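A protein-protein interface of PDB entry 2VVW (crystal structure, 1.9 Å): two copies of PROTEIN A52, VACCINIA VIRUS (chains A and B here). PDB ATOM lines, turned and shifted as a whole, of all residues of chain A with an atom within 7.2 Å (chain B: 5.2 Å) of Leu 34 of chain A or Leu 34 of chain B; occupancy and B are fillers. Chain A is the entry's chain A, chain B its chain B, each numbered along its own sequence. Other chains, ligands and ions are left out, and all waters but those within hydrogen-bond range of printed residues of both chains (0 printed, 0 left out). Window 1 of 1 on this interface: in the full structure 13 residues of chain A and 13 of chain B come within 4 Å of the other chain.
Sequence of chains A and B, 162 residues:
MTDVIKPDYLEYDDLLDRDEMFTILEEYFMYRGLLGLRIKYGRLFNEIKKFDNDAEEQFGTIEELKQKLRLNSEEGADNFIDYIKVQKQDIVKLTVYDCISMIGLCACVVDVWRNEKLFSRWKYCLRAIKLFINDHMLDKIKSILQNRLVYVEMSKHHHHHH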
ATOM      1  N   LEU A  10     -30.785  -3.126 -13.242  1.00  0.00           N
ATOM      2  CA  LEU A  10     -29.491  -2.601 -13.700  1.00  0.00           C
ATOM      3  C   LEU A  10     -29.264  -2.809 -15.194  1.00  0.00           C
ATOM      4  O   LEU A  10     -28.900  -1.867 -15.906  1.00  0.00           O
ATOM      5  CB  LEU A  10     -28.352  -3.239 -12.924  1.00  0.00           C
ATOM      6  CG  LEU A  10     -26.938  -2.717 -13.196  1.00  0.00           C
ATOM      7  CD1 LEU A  10     -26.851  -1.197 -13.137  1.00  0.00           C
ATOM      8  CD2 LEU A  10     -25.994  -3.361 -12.208  1.00  0.00           C
ATOM      9  N   GLU A  27     -33.884   1.484  -7.443  1.00  0.00           N
ATOM     10  CA  GLU A  27     -32.724   0.730  -7.906  1.00  0.00           C
ATOM     11  C   GLU A  27     -31.785   1.595  -8.719  1.00  0.00           C
ATOM     12  O   GLU A  27     -30.568   1.432  -8.638  1.00  0.00           O
ATOM     13  CB  GLU A  27     -33.158  -0.513  -8.698  1.00  0.00           C
ATOM     14  CG  GLU A  27     -33.809  -1.565  -7.815  1.00  0.00           C
ATOM     15  CD  GLU A  27     -33.775  -2.981  -8.358  1.00  0.00           C
ATOM     16  OE1 GLU A  27     -33.186  -3.240  -9.443  1.00  0.00           O
ATOM     17  OE2 GLU A  27     -34.364  -3.849  -7.668  1.00  0.00           O
ATOM     18  N   TYR A  28     -32.342   2.510  -9.515  1.00  0.00           N
ATOM     19  CA  TYR A  28     -31.529   3.461 -10.285  1.00  0.00           C
ATOM     20  C   TYR A  28     -30.638   4.323  -9.378  1.00  0.00           C
ATOM     21  O   TYR A  28     -29.425   4.426  -9.561  1.00  0.00           O
ATOM     22  CB  TYR A  28     -32.449   4.364 -11.109  1.00  0.00           C
ATOM     23  CG  TYR A  28     -31.717   5.415 -11.897  1.00  0.00           C
ATOM     24  CD1 TYR A  28     -30.943   5.059 -13.012  1.00  0.00           C
ATOM     25  CD2 TYR A  28     -31.770   6.754 -11.526  1.00  0.00           C
ATOM     26  CE1 TYR A  28     -30.264   5.999 -13.739  1.00  0.00           C
ATOM     27  CE2 TYR A  28     -31.092   7.716 -12.259  1.00  0.00           C
ATOM     28  CZ  TYR A  28     -30.334   7.331 -13.365  1.00  0.00           C
ATOM     29  OH  TYR A  28     -29.657   8.274 -14.101  1.00  0.00           O
ATOM     30  N   PHE A  29     -31.242   4.931  -8.376  1.00  0.00           N
ATOM     31  CA  PHE A  29     -30.469   5.721  -7.426  1.00  0.00           C
ATOM     32  C   PHE A  29     -29.509   4.899  -6.578  1.00  0.00           C
ATOM     33  O   PHE A  29     -28.391   5.345  -6.315  1.00  0.00           O
ATOM     34  CB  PHE A  29     -31.384   6.605  -6.582  1.00  0.00           C
ATOM     35  CG  PHE A  29     -32.042   7.692  -7.380  1.00  0.00           C
ATOM     36  CD1 PHE A  29     -31.287   8.628  -8.061  1.00  0.00           C
ATOM     37  CD2 PHE A  29     -33.411   7.776  -7.468  1.00  0.00           C
ATOM     38  CE1 PHE A  29     -31.896   9.627  -8.799  1.00  0.00           C
ATOM     39  CE2 PHE A  29     -34.015   8.771  -8.213  1.00  0.00           C
ATOM     40  CZ  PHE A  29     -33.265   9.686  -8.875  1.00  0.00           C
ATOM     41  N   MET A  30     -29.902   3.678  -6.225  1.00  0.00           N
ATOM     42  CA  MET A  30     -29.019   2.780  -5.485  1.00  0.00           C
ATOM     43  C   MET A  30     -27.800   2.461  -6.327  1.00  0.00           C
ATOM     44  O   MET A  30     -26.683   2.640  -5.882  1.00  0.00           O
ATOM     45  CB  MET A  30     -29.758   1.491  -5.138  1.00  0.00           C
ATOM     46  CG  MET A  30     -28.934   0.401  -4.515  1.00  0.00           C
ATOM     47  SD  MET A  30     -29.899  -1.114  -4.387  1.00  0.00           S
ATOM     48  CE  MET A  30     -29.896  -1.702  -6.105  1.00  0.00           C
ATOM     49  N   TYR A  31     -28.024   2.018  -7.557  1.00  0.00           N
ATOM     50  CA  TYR A  31     -26.905   1.567  -8.388  1.00  0.00           C
ATOM     51  C   TYR A  31     -26.001   2.723  -8.848  1.00  0.00           C
ATOM     52  O   TYR A  31     -24.759   2.595  -8.856  1.00  0.00           O
ATOM     53  CB  TYR A  31     -27.411   0.768  -9.588  1.00  0.00           C
ATOM     54  CG  TYR A  31     -27.789  -0.670  -9.290  1.00  0.00           C
ATOM     55  CD1 TYR A  31     -26.839  -1.578  -8.821  1.00  0.00           C
ATOM     56  CD2 TYR A  31     -29.097  -1.141  -9.508  1.00  0.00           C
ATOM     57  CE1 TYR A  31     -27.161  -2.904  -8.542  1.00  0.00           C
ATOM     58  CE2 TYR A  31     -29.430  -2.499  -9.245  1.00  0.00           C
ATOM     59  CZ  TYR A  31     -28.465  -3.357  -8.752  1.00  0.00           C
ATOM     60  OH  TYR A  31     -28.758  -4.677  -8.512  1.00  0.00           O
ATOM     61  N   ARG A  32     -26.608   3.835  -9.259  1.00  0.00           N
ATOM     62  CA  ARG A  32     -25.840   5.000  -9.663  1.00  0.00           C
ATOM     63  C   ARG A  32     -25.126   5.616  -8.452  1.00  0.00           C
ATOM     64  O   ARG A  32     -23.938   5.959  -8.517  1.00  0.00           O
ATOM     65  CB  ARG A  32     -26.728   6.030 -10.350  1.00  0.00           C
ATOM     66  CG  ARG A  32     -25.956   7.246 -10.846  1.00  0.00           C
ATOM     67  CD  ARG A  32     -26.744   8.044 -11.875  1.00  0.00           C
ATOM     68  NE  ARG A  32     -26.059   9.296 -12.195  1.00  0.00           N
ATOM     69  CZ  ARG A  32     -26.308  10.043 -13.264  1.00  0.00           C
ATOM     70  NH1 ARG A  32     -27.215   9.675 -14.146  1.00  0.00           N
ATOM     71  NH2 ARG A  32     -25.619  11.161 -13.459  1.00  0.00           N
ATOM     72  N   GLY A  33     -25.832   5.726  -7.342  1.00  0.00           N
ATOM     73  CA  GLY A  33     -25.243   6.250  -6.109  1.00  0.00           C
ATOM     74  C   GLY A  33     -24.119   5.429  -5.481  1.00  0.00           C
ATOM     75  O   GLY A  33     -23.263   5.995  -4.787  1.00  0.00           O
ATOM     76  N   LEU A  34     -24.114   4.106  -5.706  1.00  0.00           N
ATOM     77  CA  LEU A  34     -23.117   3.227  -5.097  1.00  0.00           C
ATOM     78  C   LEU A  34     -22.048   2.772  -6.081  1.00  0.00           C
ATOM     79  O   LEU A  34     -20.879   2.721  -5.706  1.00  0.00           O
ATOM     80  CB  LEU A  34     -23.771   2.014  -4.400  1.00  0.00           C
ATOM     81  CG  LEU A  34     -24.748   2.319  -3.249  1.00  0.00           C
ATOM     82  CD1 LEU A  34     -25.269   0.991  -2.575  1.00  0.00           C
ATOM     83  CD2 LEU A  34     -24.198   3.281  -2.194  1.00  0.00           C
ATOM     84  N   LEU A  35     -22.431   2.467  -7.325  1.00  0.00           N
ATOM     85  CA  LEU A  35     -21.471   1.988  -8.336  1.00  0.00           C
ATOM     86  C   LEU A  35     -21.013   3.058  -9.321  1.00  0.00           C
ATOM     87  O   LEU A  35     -19.941   2.948  -9.886  1.00  0.00           O
ATOM     88  CB  LEU A  35     -22.060   0.836  -9.151  1.00  0.00           C
ATOM     89  CG  LEU A  35     -22.559  -0.385  -8.393  1.00  0.00           C
ATOM     90  CD1 LEU A  35     -23.095  -1.378  -9.368  1.00  0.00           C
ATOM     91  CD2 LEU A  35     -21.457  -0.959  -7.534  1.00  0.00           C
ATOM     92  N   GLY A  36     -21.856   4.042  -9.591  1.00  0.00           N
ATOM     93  CA  GLY A  36     -21.537   5.057 -10.582  1.00  0.00           C
ATOM     94  C   GLY A  36     -21.837   4.645 -12.011  1.00  0.00           C
ATOM     95  O   GLY A  36     -22.568   3.693 -12.251  1.00  0.00           O
ATOM     96  N   VAL A 110     -26.566  12.685  -6.594  1.00  0.00           N
ATOM     97  CA  VAL A 110     -26.053  11.431  -6.060  1.00  0.00           C
ATOM     98  C   VAL A 110     -24.614  11.173  -6.548  1.00  0.00           C
ATOM     99  O   VAL A 110     -23.822  10.598  -5.820  1.00  0.00           O
ATOM    100  CB  VAL A 110     -27.016  10.221  -6.343  1.00  0.00           C
ATOM    101  CG1 VAL A 110     -26.713   9.534  -7.686  1.00  0.00           C
ATOM    102  CG2 VAL A 110     -26.951   9.219  -5.210  1.00  0.00           C
ATOM    103  N   ARG A 114     -21.497  10.173  -4.107  1.00  0.00           N
ATOM    104  CA  ARG A 114     -20.720   8.964  -4.341  1.00  0.00           C
ATOM    105  C   ARG A 114     -19.252   9.310  -4.364  1.00  0.00           C
ATOM    106  O   ARG A 114     -18.423   8.648  -3.711  1.00  0.00           O
ATOM    107  CB  ARG A 114     -21.131   8.317  -5.661  1.00  0.00           C
ATOM    108  CG  ARG A 114     -20.536   6.928  -5.893  1.00  0.00           C
ATOM    109  CD  ARG A 114     -20.843   6.437  -7.310  1.00  0.00           C
ATOM    110  NE  ARG A 114     -20.263   7.334  -8.306  1.00  0.00           N
ATOM    111  CZ  ARG A 114     -20.935   8.153  -9.120  1.00  0.00           C
ATOM    112  NH1 ARG A 114     -22.275   8.205  -9.141  1.00  0.00           N
ATOM    113  NH2 ARG A 114     -20.238   8.916  -9.955  1.00  0.00           N
ATOM    114  N   LEU A 118     -19.927   9.595   0.509  1.00  0.00           N
ATOM    115  CA  LEU A 118     -21.060   9.751   1.418  1.00  0.00           C
ATOM    116  C   LEU A 118     -22.142   8.800   0.941  1.00  0.00           C
ATOM    117  O   LEU A 118     -23.216   9.216   0.512  1.00  0.00           O
ATOM    118  CB  LEU A 118     -21.538  11.204   1.429  1.00  0.00           C
ATOM    119  CG  LEU A 118     -20.517  12.191   1.998  1.00  0.00           C
ATOM    120  CD1 LEU A 118     -20.862  13.654   1.726  1.00  0.00           C
ATOM    121  CD2 LEU A 118     -20.256  11.944   3.496  1.00  0.00           C
ATOM    122  N   PHE A 119     -21.864   7.503   1.066  1.00  0.00           N
ATOM    123  CA  PHE A 119     -22.576   6.504   0.288  1.00  0.00           C
ATOM    124  C   PHE A 119     -24.054   6.379   0.672  1.00  0.00           C
ATOM    125  O   PHE A 119     -24.893   6.198  -0.213  1.00  0.00           O
ATOM    126  CB  PHE A 119     -21.846   5.145   0.344  1.00  0.00           C
ATOM    127  CG  PHE A 119     -20.571   5.097  -0.476  1.00  0.00           C
ATOM    128  CD1 PHE A 119     -20.621   5.269  -1.850  1.00  0.00           C
ATOM    129  CD2 PHE A 119     -19.337   4.851   0.120  1.00  0.00           C
ATOM    130  CE1 PHE A 119     -19.453   5.216  -2.619  1.00  0.00           C
ATOM    131  CE2 PHE A 119     -18.171   4.799  -0.641  1.00  0.00           C
ATOM    132  CZ  PHE A 119     -18.237   4.977  -2.013  1.00  0.00           C
ATOM    133  N   SER A 120     -24.388   6.544   1.949  1.00  0.00           N
ATOM    134  CA  SER A 120     -25.785   6.422   2.429  1.00  0.00           C
ATOM    135  C   SER A 120     -26.743   7.569   2.048  1.00  0.00           C
ATOM    136  O   SER A 120     -27.974   7.483   2.260  1.00  0.00           O
ATOM    137  CB  SER A 120     -25.783   6.295   3.957  1.00  0.00           C
ATOM    138  OG  SER A 120     -25.279   7.471   4.555  1.00  0.00           O
ATOM    139  N   ARG A 121     -26.196   8.649   1.507  1.00  0.00           N
ATOM    140  CA  ARG A 121     -27.007   9.826   1.150  1.00  0.00           C
ATOM    141  C   ARG A 121     -27.943   9.613  -0.030  1.00  0.00           C
ATOM    142  O   ARG A 121     -28.961  10.336  -0.152  1.00  0.00           O
ATOM    143  CB  ARG A 121     -26.114  11.040   0.874  1.00  0.00           C
ATOM    144  CG  ARG A 121     -25.471  11.572   2.112  1.00  0.00           C
ATOM    145  CD  ARG A 121     -25.029  13.025   1.971  1.00  0.00           C
ATOM    146  NE  ARG A 121     -24.554  13.503   3.254  1.00  0.00           N
ATOM    147  CZ  ARG A 121     -24.028  14.705   3.482  1.00  0.00           C
ATOM    148  NH1 ARG A 121     -23.928  15.600   2.513  1.00  0.00           N
ATOM    149  NH2 ARG A 121     -23.622  15.008   4.705  1.00  0.00           N
ATOM    150  N   TRP A 122     -27.645   8.605  -0.861  1.00  0.00           N
ATOM    151  CA  TRP A 122     -28.511   8.233  -1.978  1.00  0.00           C
ATOM    152  C   TRP A 122     -29.946   8.070  -1.506  1.00  0.00           C
ATOM    153  O   TRP A 122     -30.870   8.351  -2.242  1.00  0.00           O
ATOM    154  CB  TRP A 122     -28.014   6.955  -2.685  1.00  0.00           C
ATOM    155  CG  TRP A 122     -28.260   5.671  -1.951  1.00  0.00           C
ATOM    156  CD1 TRP A 122     -27.447   5.090  -1.011  1.00  0.00           C
ATOM    157  CD2 TRP A 122     -29.374   4.796  -2.103  1.00  0.00           C
ATOM    158  NE1 TRP A 122     -27.990   3.916  -0.566  1.00  0.00           N
ATOM    159  CE2 TRP A 122     -29.174   3.705  -1.216  1.00  0.00           C
ATOM    160  CE3 TRP A 122     -30.533   4.828  -2.882  1.00  0.00           C
ATOM    161  CZ2 TRP A 122     -30.098   2.668  -1.082  1.00  0.00           C
ATOM    162  CZ3 TRP A 122     -31.453   3.793  -2.745  1.00  0.00           C
ATOM    163  CH2 TRP A 122     -31.221   2.724  -1.851  1.00  0.00           C
ATOM    164  N   PHE B  29     -26.506  -7.020   2.470  1.00  0.00           N
ATOM    165  CA  PHE B  29     -26.078  -7.617   1.196  1.00  0.00           C
ATOM    166  C   PHE B  29     -25.945  -6.589   0.085  1.00  0.00           C
ATOM    167  O   PHE B  29     -25.066  -6.715  -0.764  1.00  0.00           O
ATOM    168  CB  PHE B  29     -26.989  -8.795   0.811  1.00  0.00           C
ATOM    169  CG  PHE B  29     -26.770  -9.977   1.693  1.00  0.00           C
ATOM    170  CD1 PHE B  29     -25.547 -10.626   1.665  1.00  0.00           C
ATOM    171  CD2 PHE B  29     -27.709 -10.371   2.611  1.00  0.00           C
ATOM    172  CE1 PHE B  29     -25.283 -11.684   2.505  1.00  0.00           C
ATOM    173  CE2 PHE B  29     -27.447 -11.447   3.462  1.00  0.00           C
ATOM    174  CZ  PHE B  29     -26.223 -12.085   3.405  1.00  0.00           C
ATOM    175  N   MET B  30     -26.779  -5.551   0.125  1.00  0.00           N
ATOM    176  CA  MET B  30     -26.687  -4.456  -0.854  1.00  0.00           C
ATOM    177  C   MET B  30     -25.346  -3.747  -0.682  1.00  0.00           C
ATOM    178  O   MET B  30     -24.519  -3.694  -1.606  1.00  0.00           O
ATOM    179  CB  MET B  30     -27.836  -3.480  -0.657  1.00  0.00           C
ATOM    180  CG  MET B  30     -27.813  -2.238  -1.545  1.00  0.00           C
ATOM    181  SD  MET B  30     -29.090  -1.036  -1.089  1.00  0.00           S
ATOM    182  CE  MET B  30     -28.482  -0.422   0.526  1.00  0.00           C
ATOM    183  N   TYR B  31     -25.088  -3.246   0.520  1.00  0.00           N
ATOM    184  CA  TYR B  31     -23.855  -2.479   0.736  1.00  0.00           C
ATOM    185  C   TYR B  31     -22.596  -3.342   0.612  1.00  0.00           C
ATOM    186  O   TYR B  31     -21.630  -2.940  -0.041  1.00  0.00           O
ATOM    187  CB  TYR B  31     -23.907  -1.769   2.083  1.00  0.00           C
ATOM    188  CG  TYR B  31     -24.772  -0.524   2.096  1.00  0.00           C
ATOM    189  CD1 TYR B  31     -24.483   0.564   1.256  1.00  0.00           C
ATOM    190  CD2 TYR B  31     -25.833  -0.400   2.980  1.00  0.00           C
ATOM    191  CE1 TYR B  31     -25.265   1.731   1.280  1.00  0.00           C
ATOM    192  CE2 TYR B  31     -26.589   0.747   3.023  1.00  0.00           C
ATOM    193  CZ  TYR B  31     -26.318   1.800   2.164  1.00  0.00           C
ATOM    194  OH  TYR B  31     -27.102   2.917   2.218  1.00  0.00           O
ATOM    195  N   ARG B  32     -22.595  -4.533   1.206  1.00  0.00           N
ATOM    196  CA  ARG B  32     -21.439  -5.400   1.077  1.00  0.00           C
ATOM    197  C   ARG B  32     -21.291  -5.831  -0.389  1.00  0.00           C
ATOM    198  O   ARG B  32     -20.185  -5.840  -0.936  1.00  0.00           O
ATOM    199  CB  ARG B  32     -21.560  -6.623   2.003  1.00  0.00           C
ATOM    200  CG  ARG B  32     -20.385  -7.550   1.889  1.00  0.00           C
ATOM    201  CD  ARG B  32     -20.135  -8.345   3.145  1.00  0.00           C
ATOM    202  NE  ARG B  32     -19.047  -9.294   2.927  1.00  0.00           N
ATOM    203  CZ  ARG B  32     -18.533 -10.108   3.844  1.00  0.00           C
ATOM    204  NH1 ARG B  32     -18.956 -10.069   5.091  1.00  0.00           N
ATOM    205  NH2 ARG B  32     -17.544 -10.927   3.505  1.00  0.00           N
ATOM    206  N   GLY B  33     -22.407  -6.153  -1.033  1.00  0.00           N
ATOM    207  CA  GLY B  33     -22.353  -6.626  -2.413  1.00  0.00           C
ATOM    208  C   GLY B  33     -21.956  -5.584  -3.435  1.00  0.00           C
ATOM    209  O   GLY B  33     -21.448  -5.926  -4.491  1.00  0.00           O
ATOM    210  N   LEU B  34     -22.237  -4.315  -3.156  1.00  0.00           N
ATOM    211  CA  LEU B  34     -21.958  -3.244  -4.135  1.00  0.00           C
ATOM    212  C   LEU B  34     -20.722  -2.417  -3.793  1.00  0.00           C
ATOM    213  O   LEU B  34     -20.007  -1.989  -4.700  1.00  0.00           O
ATOM    214  CB  LEU B  34     -23.174  -2.336  -4.306  1.00  0.00           C
ATOM    215  CG  LEU B  34     -24.471  -3.077  -4.698  1.00  0.00           C
ATOM    216  CD1 LEU B  34     -25.646  -2.097  -4.813  1.00  0.00           C
ATOM    217  CD2 LEU B  34     -24.301  -3.869  -5.997  1.00  0.00           C
ATOM    218  N   LEU B  35     -20.473  -2.192  -2.502  1.00  0.00           N
ATOM    219  CA  LEU B  35     -19.341  -1.362  -2.060  1.00  0.00           C
ATOM    220  C   LEU B  35     -18.153  -2.163  -1.575  1.00  0.00           C
ATOM    221  O   LEU B  35     -17.023  -1.751  -1.757  1.00  0.00           O
ATOM    222  CB  LEU B  35     -19.756  -0.394  -0.948  1.00  0.00           C
ATOM    223  CG  LEU B  35     -20.751   0.702  -1.328  1.00  0.00           C
ATOM    224  CD1 LEU B  35     -21.007   1.569  -0.107  1.00  0.00           C
ATOM    225  CD2 LEU B  35     -20.253   1.535  -2.490  1.00  0.00           C
ATOM    226  N   GLY B  36     -18.416  -3.284  -0.921  1.00  0.00           N
ATOM    227  CA  GLY B  36     -17.356  -4.128  -0.416  1.00  0.00           C
ATOM    228  C   GLY B  36     -17.000  -3.744   1.008  1.00  0.00           C
ATOM    229  O   GLY B  36     -17.701  -2.965   1.653  1.00  0.00           O
ATOM    230  N   ARG B 114     -18.870  -9.507  -6.509  1.00  0.00           N
ATOM    231  CA  ARG B 114     -18.511  -8.089  -6.570  1.00  0.00           C
ATOM    232  C   ARG B 114     -17.159  -7.902  -7.218  1.00  0.00           C
ATOM    233  O   ARG B 114     -16.993  -7.042  -8.092  1.00  0.00           O
ATOM    234  CB  ARG B 114     -18.462  -7.477  -5.175  1.00  0.00           C
ATOM    235  CG  ARG B 114     -18.247  -5.967  -5.162  1.00  0.00           C
ATOM    236  CD  ARG B 114     -18.057  -5.485  -3.746  1.00  0.00           C
ATOM    237  NE  ARG B 114     -16.868  -6.128  -3.193  1.00  0.00           N
ATOM    238  CZ  ARG B 114     -16.840  -7.012  -2.195  1.00  0.00           C
ATOM    239  NH1 ARG B 114     -15.674  -7.537  -1.857  1.00  0.00           N
ATOM    240  NH2 ARG B 114     -17.931  -7.347  -1.507  1.00  0.00           N
ATOM    241  N   PHE B 119     -22.486  -7.335 -10.374  1.00  0.00           N
ATOM    242  CA  PHE B 119     -23.042  -6.571  -9.261  1.00  0.00           C
ATOM    243  C   PHE B 119     -24.469  -6.956  -8.916  1.00  0.00           C
ATOM    244  O   PHE B 119     -24.815  -7.078  -7.734  1.00  0.00           O
ATOM    245  CB  PHE B 119     -22.918  -5.078  -9.537  1.00  0.00           C
ATOM    246  CG  PHE B 119     -21.496  -4.584  -9.504  1.00  0.00           C
ATOM    247  CD1 PHE B 119     -20.760  -4.635  -8.328  1.00  0.00           C
ATOM    248  CD2 PHE B 119     -20.893  -4.064 -10.640  1.00  0.00           C
ATOM    249  CE1 PHE B 119     -19.445  -4.173  -8.282  1.00  0.00           C
ATOM    250  CE2 PHE B 119     -19.567  -3.602 -10.596  1.00  0.00           C
ATOM    251  CZ  PHE B 119     -18.854  -3.658  -9.417  1.00  0.00           C
ATOM    252  N   TRP B 122     -26.020  -9.856  -6.148  1.00  0.00           N
ATOM    253  CA  TRP B 122     -26.334  -9.691  -4.734  1.00  0.00           C
ATOM    254  C   TRP B 122     -27.810 -10.027  -4.424  1.00  0.00           C
ATOM    255  O   TRP B 122     -28.129 -10.459  -3.326  1.00  0.00           O
ATOM    256  CB  TRP B 122     -25.973  -8.278  -4.266  1.00  0.00           C
ATOM    257  CG  TRP B 122     -26.916  -7.225  -4.667  1.00  0.00           C
ATOM    258  CD1 TRP B 122     -26.947  -6.531  -5.837  1.00  0.00           C
ATOM    259  CD2 TRP B 122     -27.982  -6.721  -3.876  1.00  0.00           C
ATOM    260  NE1 TRP B 122     -27.978  -5.632  -5.833  1.00  0.00           N
ATOM    261  CE2 TRP B 122     -28.628  -5.720  -4.632  1.00  0.00           C
ATOM    262  CE3 TRP B 122     -28.465  -7.030  -2.606  1.00  0.00           C
ATOM    263  CZ2 TRP B 122     -29.735  -5.026  -4.154  1.00  0.00           C
ATOM    264  CZ3 TRP B 122     -29.554  -6.341  -2.130  1.00  0.00           C
ATOM    265  CH2 TRP B 122     -30.179  -5.343  -2.902  1.00  0.00           C
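The side-chain sulfur of Met 30 of chain A sits close to the side-chain sulfur of Met 30 of chain B (3.4 Å). OH of Tyr 31 of chain B is in hydrogen-bond range of NE1 of Trp 122 of chain A (3.1 Å). The indole nitrogen (NE1) of Trp 122 of chain B lies within hydrogen-bond range of the side-chain hydroxyl (OH) of Tyr 31 of chain A, at 2.9 Å.
The backbone carbonyl oxygen (O) of Tyr 31 of chain B is in hydrogen-bond range of the backbone NH (N) of Gly 36 of chain B (3.4 Å). The backbone carbonyl oxygen (O) of Tyr 31 of chain A lies within hydrogen-bond range of the backbone NH (N) of Gly 36 of chain A (3.3 Å).
Met 30 of chain A touches Trp 122 of chain B. Tyr 31 of chain A touches Leu 34 of chain B. CD1 of Leu 34 of chain A touches CE1 of Tyr 31 of chain B, 3.9 Å away. Leu 34 of chain B touches Leu 34 of chain A (CD1 to CD1, 3.8 Å). Leu 34 of chain A touches Leu 35 of chain B (O to CD2, 3.5 Å). Leu 35 of chain A touches Leu 34 of chain B. CG of Phe 119 of chain B touches CD1 of Leu 35 of chain A, at 3.6 Å. CG of Phe 119 of chain A touches CD1 of Leu 35 of chain B (3.6 Å). Ser 120 of chain A touches Tyr 31 of chain B. Trp 122 of chain A touches Met 30 of chain B.
Of the printed residues of chain B, Met 30 of chain A touches Met 30 (3.4 Å) and Trp 122 (3.9 Å). Printed residues of chain B within 4 Å of Tyr 31 of chain A: Leu 34 and Trp 122. Of chain B, only Tyr 31 (3.9 Å), Leu 34 (3.8 Å) and Leu 35 (3.5 Å) come within 4 Å of Leu 34 of chain A. Printed residues of chain B within 4 Å of Leu 35 of chain A: Leu 34 (3.3 Å) and Phe 119 (3.6 Å). Of the printed residues of chain B, Phe 119 of chain A touches Leu 35 (3.6 Å). Leu 34 of chain B touches three residues of chain A. The nearest residue of chain B that does not touch Leu 34 of chain A is Met 30 of chain B (4.2 Å). The nearest residue of chain A that does not touch Leu 34 of chain B is Met 30 of chain A (4.1 Å). The nearest printed residue of chain A that does not touch Trp 122 of chain B is Glu 27 of chain A (5.9 Å).
Among the printed residues, 13 pairs touch across the chains. Among the printed residues, no Asp or Glu carboxylate lies within 4 Å of a Lys or Arg side-chain nitrogen of the other chain.
Met 30 of chain B touches its own counterpart, Met 30 of chain A. Tyr 31 of chain A touches Leu 34 of chain B, and with the chains exchanged Leu 34 of chain A touches Tyr 31 of chain B. Tyr 31 of chain A touches Trp 122 of chain B, and with the chains exchanged Trp 122 of chain A touches Tyr 31 of chain B. Leu 35 of chain A touches Phe 119 of chain B, and with the chains exchanged Phe 119 of chain A touches Leu 35 of chain B. Of the 13 pairs that touch across the chains among the printed residues, 12 have their exchanged pair printed and touching as well.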
